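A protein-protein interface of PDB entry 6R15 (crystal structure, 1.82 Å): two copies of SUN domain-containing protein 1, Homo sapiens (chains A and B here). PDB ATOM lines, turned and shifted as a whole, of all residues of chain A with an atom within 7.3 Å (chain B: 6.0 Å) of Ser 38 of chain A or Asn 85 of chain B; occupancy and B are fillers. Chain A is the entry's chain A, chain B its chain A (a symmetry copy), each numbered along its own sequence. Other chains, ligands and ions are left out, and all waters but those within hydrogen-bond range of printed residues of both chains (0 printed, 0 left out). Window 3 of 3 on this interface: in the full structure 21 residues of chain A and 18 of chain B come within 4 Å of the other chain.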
ATOM      1  N   ALA A  35     -25.321 -10.612  -9.555  1.00  0.00           N
ATOM      2  CA  ALA A  35     -24.495 -11.819  -9.719  1.00  0.00           C
ATOM      3  C   ALA A  35     -24.857 -12.652 -10.951  1.00  0.00           C
ATOM      4  O   ALA A  35     -24.076 -13.558 -11.310  1.00  0.00           O
ATOM      5  CB  ALA A  35     -24.604 -12.730  -8.497  1.00  0.00           C
ATOM      6  N   LEU A  36     -26.023 -12.405 -11.569  1.00  0.00           N
ATOM      7  CA  LEU A  36     -26.508 -13.236 -12.665  1.00  0.00           C
ATOM      8  C   LEU A  36     -25.495 -13.319 -13.812  1.00  0.00           C
ATOM      9  O   LEU A  36     -25.062 -12.297 -14.345  1.00  0.00           O
ATOM     10  CB  LEU A  36     -27.832 -12.662 -13.180  1.00  0.00           C
ATOM     11  CG  LEU A  36     -28.550 -13.423 -14.301  1.00  0.00           C
ATOM     12  CD1 LEU A  36     -29.208 -14.698 -13.736  1.00  0.00           C
ATOM     13  CD2 LEU A  36     -29.583 -12.466 -15.009  1.00  0.00           C
ATOM     14  N   GLU A  37     -25.182 -14.553 -14.253  1.00  0.00           N
ATOM     15  CA  GLU A  37     -24.108 -14.713 -15.235  1.00  0.00           C
ATOM     16  C   GLU A  37     -24.460 -14.038 -16.573  1.00  0.00           C
ATOM     17  O   GLU A  37     -23.615 -13.346 -17.166  1.00  0.00           O
ATOM     18  CB  GLU A  37     -23.761 -16.193 -15.440  1.00  0.00           C
ATOM     19  CG  GLU A  37     -22.487 -16.415 -16.283  1.00  0.00           C
ATOM     20  CD  GLU A  37     -22.058 -17.882 -16.413  1.00  0.00           C
ATOM     21  OE1 GLU A  37     -22.696 -18.640 -17.193  1.00  0.00           O
ATOM     22  OE2 GLU A  37     -21.049 -18.260 -15.757  1.00  0.00           O
ATOM     23  N   SER A  38     -25.697 -14.246 -17.089  1.00  0.00           N
ATOM     24  CA  SER A  38     -26.026 -13.692 -18.400  1.00  0.00           C
ATOM     25  C   SER A  38     -25.964 -12.145 -18.386  1.00  0.00           C
ATOM     26  O   SER A  38     -25.693 -11.528 -19.431  1.00  0.00           O
ATOM     27  CB  SER A  38     -27.413 -14.206 -18.857  1.00  0.00           C
ATOM     28  OG  SER A  38     -28.430 -13.739 -17.973  1.00  0.00           O
ATOM     29  N   GLY A  39     -26.149 -11.536 -17.211  1.00  0.00           N
ATOM     30  CA  GLY A  39     -26.122 -10.101 -17.040  1.00  0.00           C
ATOM     31  C   GLY A  39     -24.777  -9.483 -16.714  1.00  0.00           C
ATOM     32  O   GLY A  39     -24.699  -8.262 -16.557  1.00  0.00           O
ATOM     33  N   GLY A  40     -23.695 -10.258 -16.653  1.00  0.00           N
ATOM     34  CA  GLY A  40     -22.356  -9.711 -16.391  1.00  0.00           C
ATOM     35  C   GLY A  40     -21.650 -10.246 -15.145  1.00  0.00           C
ATOM     36  O   GLY A  40     -20.475  -9.885 -14.933  1.00  0.00           O
ATOM     37  N   GLY A  41     -22.284 -11.101 -14.308  1.00  0.00           N
ATOM     38  CA  GLY A  41     -21.595 -11.731 -13.167  1.00  0.00           C
ATOM     39  C   GLY A  41     -20.750 -12.939 -13.551  1.00  0.00           C
ATOM     40  O   GLY A  41     -20.945 -13.545 -14.614  1.00  0.00           O
ATOM     41  N   ILE A  77     -25.147 -19.216 -10.458  1.00  0.00           N
ATOM     42  CA  ILE A  77     -25.587 -17.904 -10.934  1.00  0.00           C
ATOM     43  C   ILE A  77     -26.347 -18.038 -12.267  1.00  0.00           C
ATOM     44  O   ILE A  77     -26.259 -17.166 -13.164  1.00  0.00           O
ATOM     45  CB  ILE A  77     -24.395 -16.933 -11.030  1.00  0.00           C
ATOM     46  CG1 ILE A  77     -23.221 -17.492 -11.843  1.00  0.00           C
ATOM     47  CG2 ILE A  77     -23.874 -16.576  -9.580  1.00  0.00           C
ATOM     48  CD1 ILE A  77     -22.138 -16.392 -12.176  1.00  0.00           C
ATOM     49  N   GLN A  78     -27.083 -19.172 -12.416  1.00  0.00           N
ATOM     50  CA  GLN A  78     -27.975 -19.450 -13.545  1.00  0.00           C
ATOM     51  C   GLN A  78     -29.390 -19.761 -13.008  1.00  0.00           C
ATOM     52  O   GLN A  78     -29.513 -20.370 -11.942  1.00  0.00           O
ATOM     53  CB  GLN A  78     -27.417 -20.645 -14.397  1.00  0.00           C
ATOM     54  CG  GLN A  78     -26.025 -20.304 -15.055  1.00  0.00           C
ATOM     55  CD  GLN A  78     -25.323 -21.486 -15.756  1.00  0.00           C
ATOM     56  OE1 GLN A  78     -25.797 -22.627 -15.716  1.00  0.00           O
ATOM     57  NE2 GLN A  78     -24.187 -21.204 -16.415  1.00  0.00           N
ATOM     58  N   PRO A  79     -30.464 -19.349 -13.699  1.00  0.00           N
ATOM     59  CA  PRO A  79     -31.788 -19.320 -13.028  1.00  0.00           C
ATOM     60  C   PRO A  79     -32.560 -20.650 -12.904  1.00  0.00           C
ATOM     61  O   PRO A  79     -33.426 -20.745 -12.011  1.00  0.00           O
ATOM     62  CB  PRO A  79     -32.579 -18.298 -13.866  1.00  0.00           C
ATOM     63  CG  PRO A  79     -31.927 -18.351 -15.242  1.00  0.00           C
ATOM     64  CD  PRO A  79     -30.451 -18.583 -14.963  1.00  0.00           C
ATOM     65  N   GLN B  71     -23.540 -13.101 -28.285  1.00  0.00           N
ATOM     66  CA  GLN B  71     -24.816 -13.714 -28.639  1.00  0.00           C
ATOM     67  C   GLN B  71     -25.080 -13.643 -30.143  1.00  0.00           C
ATOM     68  O   GLN B  71     -24.766 -12.637 -30.797  1.00  0.00           O
ATOM     69  CB  GLN B  71     -25.980 -13.027 -27.914  1.00  0.00           C
ATOM     70  CG  GLN B  71     -25.903 -13.030 -26.383  1.00  0.00           C
ATOM     71  CD  GLN B  71     -26.308 -14.344 -25.749  1.00  0.00           C
ATOM     72  OE1 GLN B  71     -26.641 -15.330 -26.425  1.00  0.00           O
ATOM     73  NE2 GLN B  71     -26.268 -14.370 -24.423  1.00  0.00           N
ATOM     74  N   VAL B  75     -30.816 -15.728 -31.166  1.00  0.00           N
ATOM     75  CA  VAL B  75     -31.453 -15.613 -29.849  1.00  0.00           C
ATOM     76  C   VAL B  75     -32.763 -14.801 -29.931  1.00  0.00           C
ATOM     77  O   VAL B  75     -33.626 -14.924 -29.021  1.00  0.00           O
ATOM     78  CB  VAL B  75     -30.539 -15.025 -28.733  1.00  0.00           C
ATOM     79  CG1 VAL B  75     -29.282 -15.868 -28.576  1.00  0.00           C
ATOM     80  CG2 VAL B  75     -30.247 -13.533 -28.908  1.00  0.00           C
ATOM     81  N   ASP B  80     -36.124 -17.423 -23.910  1.00  0.00           N
ATOM     82  CA  ASP B  80     -35.434 -16.864 -22.717  1.00  0.00           C
ATOM     83  C   ASP B  80     -35.163 -15.371 -22.869  1.00  0.00           C
ATOM     84  O   ASP B  80     -34.564 -14.935 -23.865  1.00  0.00           O
ATOM     85  CB  ASP B  80     -34.111 -17.620 -22.521  1.00  0.00           C
ATOM     86  CG  ASP B  80     -33.317 -17.197 -21.281  1.00  0.00           C
ATOM     87  OD1 ASP B  80     -33.221 -16.000 -20.951  1.00  0.00           O
ATOM     88  OD2 ASP B  80     -32.725 -18.112 -20.666  1.00  0.00           O
ATOM     89  N   ILE B  81     -35.631 -14.558 -21.903  1.00  0.00           N
ATOM     90  CA  ILE B  81     -35.337 -13.120 -21.940  1.00  0.00           C
ATOM     91  C   ILE B  81     -34.755 -12.602 -20.616  1.00  0.00           C
ATOM     92  O   ILE B  81     -34.988 -11.442 -20.227  1.00  0.00           O
ATOM     93  CB  ILE B  81     -36.577 -12.297 -22.340  1.00  0.00           C
ATOM     94  CG1 ILE B  81     -37.722 -12.519 -21.356  1.00  0.00           C
ATOM     95  CG2 ILE B  81     -37.008 -12.648 -23.763  1.00  0.00           C
ATOM     96  CD1 ILE B  81     -38.784 -11.428 -21.449  1.00  0.00           C
ATOM     97  N   TYR B  82     -33.970 -13.433 -19.922  1.00  0.00           N
ATOM     98  CA  TYR B  82     -33.162 -12.926 -18.829  1.00  0.00           C
ATOM     99  C   TYR B  82     -32.205 -11.854 -19.371  1.00  0.00           C
ATOM    100  O   TYR B  82     -31.792 -11.919 -20.544  1.00  0.00           O
ATOM    101  CB  TYR B  82     -32.385 -14.076 -18.158  1.00  0.00           C
ATOM    102  CG  TYR B  82     -33.247 -14.802 -17.134  1.00  0.00           C
ATOM    103  CD1 TYR B  82     -34.173 -15.773 -17.537  1.00  0.00           C
ATOM    104  CD2 TYR B  82     -33.199 -14.461 -15.778  1.00  0.00           C
ATOM    105  CE1 TYR B  82     -35.012 -16.418 -16.593  1.00  0.00           C
ATOM    106  CE2 TYR B  82     -34.051 -15.096 -14.839  1.00  0.00           C
ATOM    107  CZ  TYR B  82     -34.951 -16.031 -15.267  1.00  0.00           C
ATOM    108  OH  TYR B  82     -35.776 -16.614 -14.363  1.00  0.00           O
ATOM    109  N   PRO B  83     -31.846 -10.854 -18.553  1.00  0.00           N
ATOM    110  CA  PRO B  83     -30.875  -9.834 -18.986  1.00  0.00           C
ATOM    111  C   PRO B  83     -29.648 -10.427 -19.681  1.00  0.00           C
ATOM    112  O   PRO B  83     -28.997 -11.344 -19.174  1.00  0.00           O
ATOM    113  CB  PRO B  83     -30.485  -9.137 -17.670  1.00  0.00           C
ATOM    114  CG  PRO B  83     -31.762  -9.250 -16.804  1.00  0.00           C
ATOM    115  CD  PRO B  83     -32.350 -10.602 -17.175  1.00  0.00           C
ATOM    116  N   GLY B  84     -29.324  -9.863 -20.860  1.00  0.00           N
ATOM    117  CA  GLY B  84     -28.182 -10.290 -21.664  1.00  0.00           C
ATOM    118  C   GLY B  84     -28.491 -11.324 -22.735  1.00  0.00           C
ATOM    119  O   GLY B  84     -27.639 -11.562 -23.613  1.00  0.00           O
ATOM    120  N   ASN B  85     -29.672 -11.949 -22.698  1.00  0.00           N
ATOM    121  CA  ASN B  85     -30.067 -12.949 -23.703  1.00  0.00           C
ATOM    122  C   ASN B  85     -30.752 -12.279 -24.904  1.00  0.00           C
ATOM    123  O   ASN B  85     -31.932 -12.496 -25.197  1.00  0.00           O
ATOM    124  CB  ASN B  85     -30.941 -14.009 -23.035  1.00  0.00           C
ATOM    125  CG  ASN B  85     -30.110 -14.905 -22.097  1.00  0.00           C
ATOM    126  OD1 ASN B  85     -28.899 -15.078 -22.299  1.00  0.00           O
ATOM    127  ND2 ASN B  85     -30.724 -15.426 -21.061  1.00  0.00           N
ATOM    128  N   CYS B  86     -29.954 -11.451 -25.597  1.00  0.00           N
ATOM    129  CA  CYS B  86     -30.403 -10.546 -26.639  1.00  0.00           C
ATOM    130  C   CYS B  86     -29.303 -10.430 -27.689  1.00  0.00           C
ATOM    131  O   CYS B  86     -28.123 -10.641 -27.402  1.00  0.00           O
ATOM    132  CB  CYS B  86     -30.720  -9.145 -26.079  1.00  0.00           C
ATOM    133  SG  CYS B  86     -29.401  -8.423 -25.005  1.00  0.00           S
ATOM    134  N   TRP B  87     -29.689 -10.041 -28.908  1.00  0.00           N
ATOM    135  CA  TRP B  87     -28.738  -9.773 -29.987  1.00  0.00           C
ATOM    136  C   TRP B  87     -28.431  -8.279 -30.017  1.00  0.00           C
ATOM    137  O   TRP B  87     -29.348  -7.454 -30.095  1.00  0.00           O
ATOM    138  CB  TRP B  87     -29.300 -10.234 -31.341  1.00  0.00           C
ATOM    139  CG  TRP B  87     -28.458  -9.871 -32.535  1.00  0.00           C
ATOM    140  CD1 TRP B  87     -27.155 -10.184 -32.711  1.00  0.00           C
ATOM    141  CD2 TRP B  87     -28.862  -9.140 -33.713  1.00  0.00           C
ATOM    142  NE1 TRP B  87     -26.704  -9.687 -33.919  1.00  0.00           N
ATOM    143  CE2 TRP B  87     -27.733  -9.050 -34.551  1.00  0.00           C
ATOM    144  CE3 TRP B  87     -30.058  -8.561 -34.141  1.00  0.00           C
ATOM    145  CZ2 TRP B  87     -27.762  -8.392 -35.801  1.00  0.00           C
ATOM    146  CZ3 TRP B  87     -30.083  -7.889 -35.398  1.00  0.00           C
ATOM    147  CH2 TRP B  87     -28.944  -7.830 -36.199  1.00  0.00           C
ATOM    148  N   LEU B 192     -31.876  -6.511 -29.020  1.00  0.00           N
ATOM    149  CA  LEU B 192     -33.180  -7.101 -29.329  1.00  0.00           C
ATOM    150  C   LEU B 192     -33.341  -8.407 -28.559  1.00  0.00           C
ATOM    151  O   LEU B 192     -32.581  -9.355 -28.782  1.00  0.00           O
ATOM    152  CB  LEU B 192     -33.329  -7.374 -30.828  1.00  0.00           C
ATOM    153  CG  LEU B 192     -33.366  -6.200 -31.799  1.00  0.00           C
ATOM    154  CD1 LEU B 192     -33.497  -6.717 -33.241  1.00  0.00           C
ATOM    155  CD2 LEU B 192     -34.498  -5.270 -31.433  1.00  0.00           C
ATOM    156  N   TYR B 193     -34.368  -8.482 -27.711  1.00  0.00           N
ATOM    157  CA  TYR B 193     -34.595  -9.699 -26.918  1.00  0.00           C
ATOM    158  C   TYR B 193     -35.466 -10.761 -27.600  1.00  0.00           C
ATOM    159  O   TYR B 193     -35.090 -11.943 -27.615  1.00  0.00           O
ATOM    160  CB  TYR B 193     -35.212  -9.323 -25.548  1.00  0.00           C
ATOM    161  CG  TYR B 193     -34.166  -8.870 -24.536  1.00  0.00           C
ATOM    162  CD1 TYR B 193     -33.730  -7.548 -24.505  1.00  0.00           C
ATOM    163  CD2 TYR B 193     -33.563  -9.776 -23.653  1.00  0.00           C
ATOM    164  CE1 TYR B 193     -32.723  -7.111 -23.596  1.00  0.00           C
ATOM    165  CE2 TYR B 193     -32.571  -9.373 -22.734  1.00  0.00           C
ATOM    166  CZ  TYR B 193     -32.149  -8.030 -22.714  1.00  0.00           C
ATOM    167  OH  TYR B 193     -31.154  -7.638 -21.800  1.00  0.00           O
ATOM    168  N   ARG B 194     -36.647 -10.404 -28.101  1.00  0.00           N
ATOM    169  CA  ARG B 194     -37.478 -11.360 -28.828  1.00  0.00           C
ATOM    170  C   ARG B 194     -38.460 -10.634 -29.752  1.00  0.00           C
ATOM    171  O   ARG B 194     -39.047  -9.599 -29.380  1.00  0.00           O
ATOM    172  CB  ARG B 194     -38.258 -12.295 -27.865  1.00  0.00           C
ATOM    173  CG  ARG B 194     -39.020 -13.395 -28.644  1.00  0.00           C
ATOM    174  CD  ARG B 194     -39.485 -14.552 -27.814  1.00  0.00           C
ATOM    175  NE  ARG B 194     -40.388 -15.407 -28.576  1.00  0.00           N
ATOM    176  CZ  ARG B 194     -41.345 -16.145 -28.031  1.00  0.00           C
ATOM    177  NH1 ARG B 194     -41.508 -16.205 -26.704  1.00  0.00           N
ATOM    178  NH2 ARG B 194     -42.166 -16.864 -28.805  1.00  0.00           N
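No position is printed for both chains.
Of the 7 pairs that touch across the chains among the printed residues, none has its exchanged pair printed and touching as well.
Among the printed residues, merely in contact across the chains: Ser 38 of chain A with Gly 84 of chain B (3.6 Å), Pro 79 of chain A with Tyr 82 of chain B (3.6 Å), Ser 38 of chain A with Asn 85 of chain B (3.8 Å), Ser 38 of chain A with Tyr 82 of chain B (3.97 Å) and Leu 36 of chain A with Pro 83 of chain B (3.98 Å).
Hydrophobic or aromatic side chains of chain A that line the printed part of chain B: Leu 36 and Pro 79.
Of the 13 printed residues of chain B, 4 touch a printed residue of chain A.
Printed residues of chain B that touch a printed residue of chain A: Tyr 82, Pro 83, Gly 84 and Asn 85.
Among the printed residues, no Asp or Glu carboxylate lies within 4 Å of a Lys or Arg side-chain nitrogen of the other chain.
Ser 38 of chain A touches just these residues of chain B: Tyr 82 (3.97 Å), Pro 83 (2.7 Å), Gly 84 (3.6 Å) and Asn 85 (3.8 Å).
Of the printed residues of chain B, Gly 39 of chain A touches Pro 83 (3.5 Å).
Val 75 of chain B touches none of the printed residues of chain A.
Asp 80 of chain B touches none of the printed residues of chain A.
Of the printed residues of chain A, Pro 83 of chain B touches Leu 36, Ser 38 and Gly 39.
Of the printed residues of chain A, Gly 84 of chain B touches Ser 38.
Of chain A, only Ser 38 comes within 4 Å of Asn 85 of chain B.
The nearest residue of chain A that does not touch Asn 85 of chain B is Gly 39 of chain A (6.5 Å).
The nearest printed residue of chain B that does not touch Pro 79 of chain A is Asp 80 of chain B (5.5 Å).
O of Pro 83 of chain B lies within hydrogen-bond range of OG of Ser 38 of chain A (2.7 Å).
N of Gly 39 of chain A sits at hydrogen-bond distance from O of Pro 83 of chain B.
O of Leu 36 of chain A is in hydrogen-bond range of N of Gly 41 of chain A (3.0 Å).
The side-chain amide nitrogen (NE2) of Gln 71 of chain B sits at hydrogen-bond distance from the backbone carbonyl oxygen (O) of Gly 84 of chain B.
NE2 of Gln 71 of chain B lies within hydrogen-bond range of OD1 of Asn 85 of chain B.
The side-chain carboxylate (OD1) of Asp 80 of chain B sits at hydrogen-bond distance from the backbone NH (N) of Tyr 82 of chain B (2.9 Å).
The side-chain carboxylate (OD1) of Asp 80 of chain B sits at hydrogen-bond distance from the side-chain amide nitrogen (ND2) of Asn 85 of chain B (2.6 Å).
N of Gly 84 of chain B lies within hydrogen-bond range of OH of Tyr 193 of chain B, 3.0 Å away.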
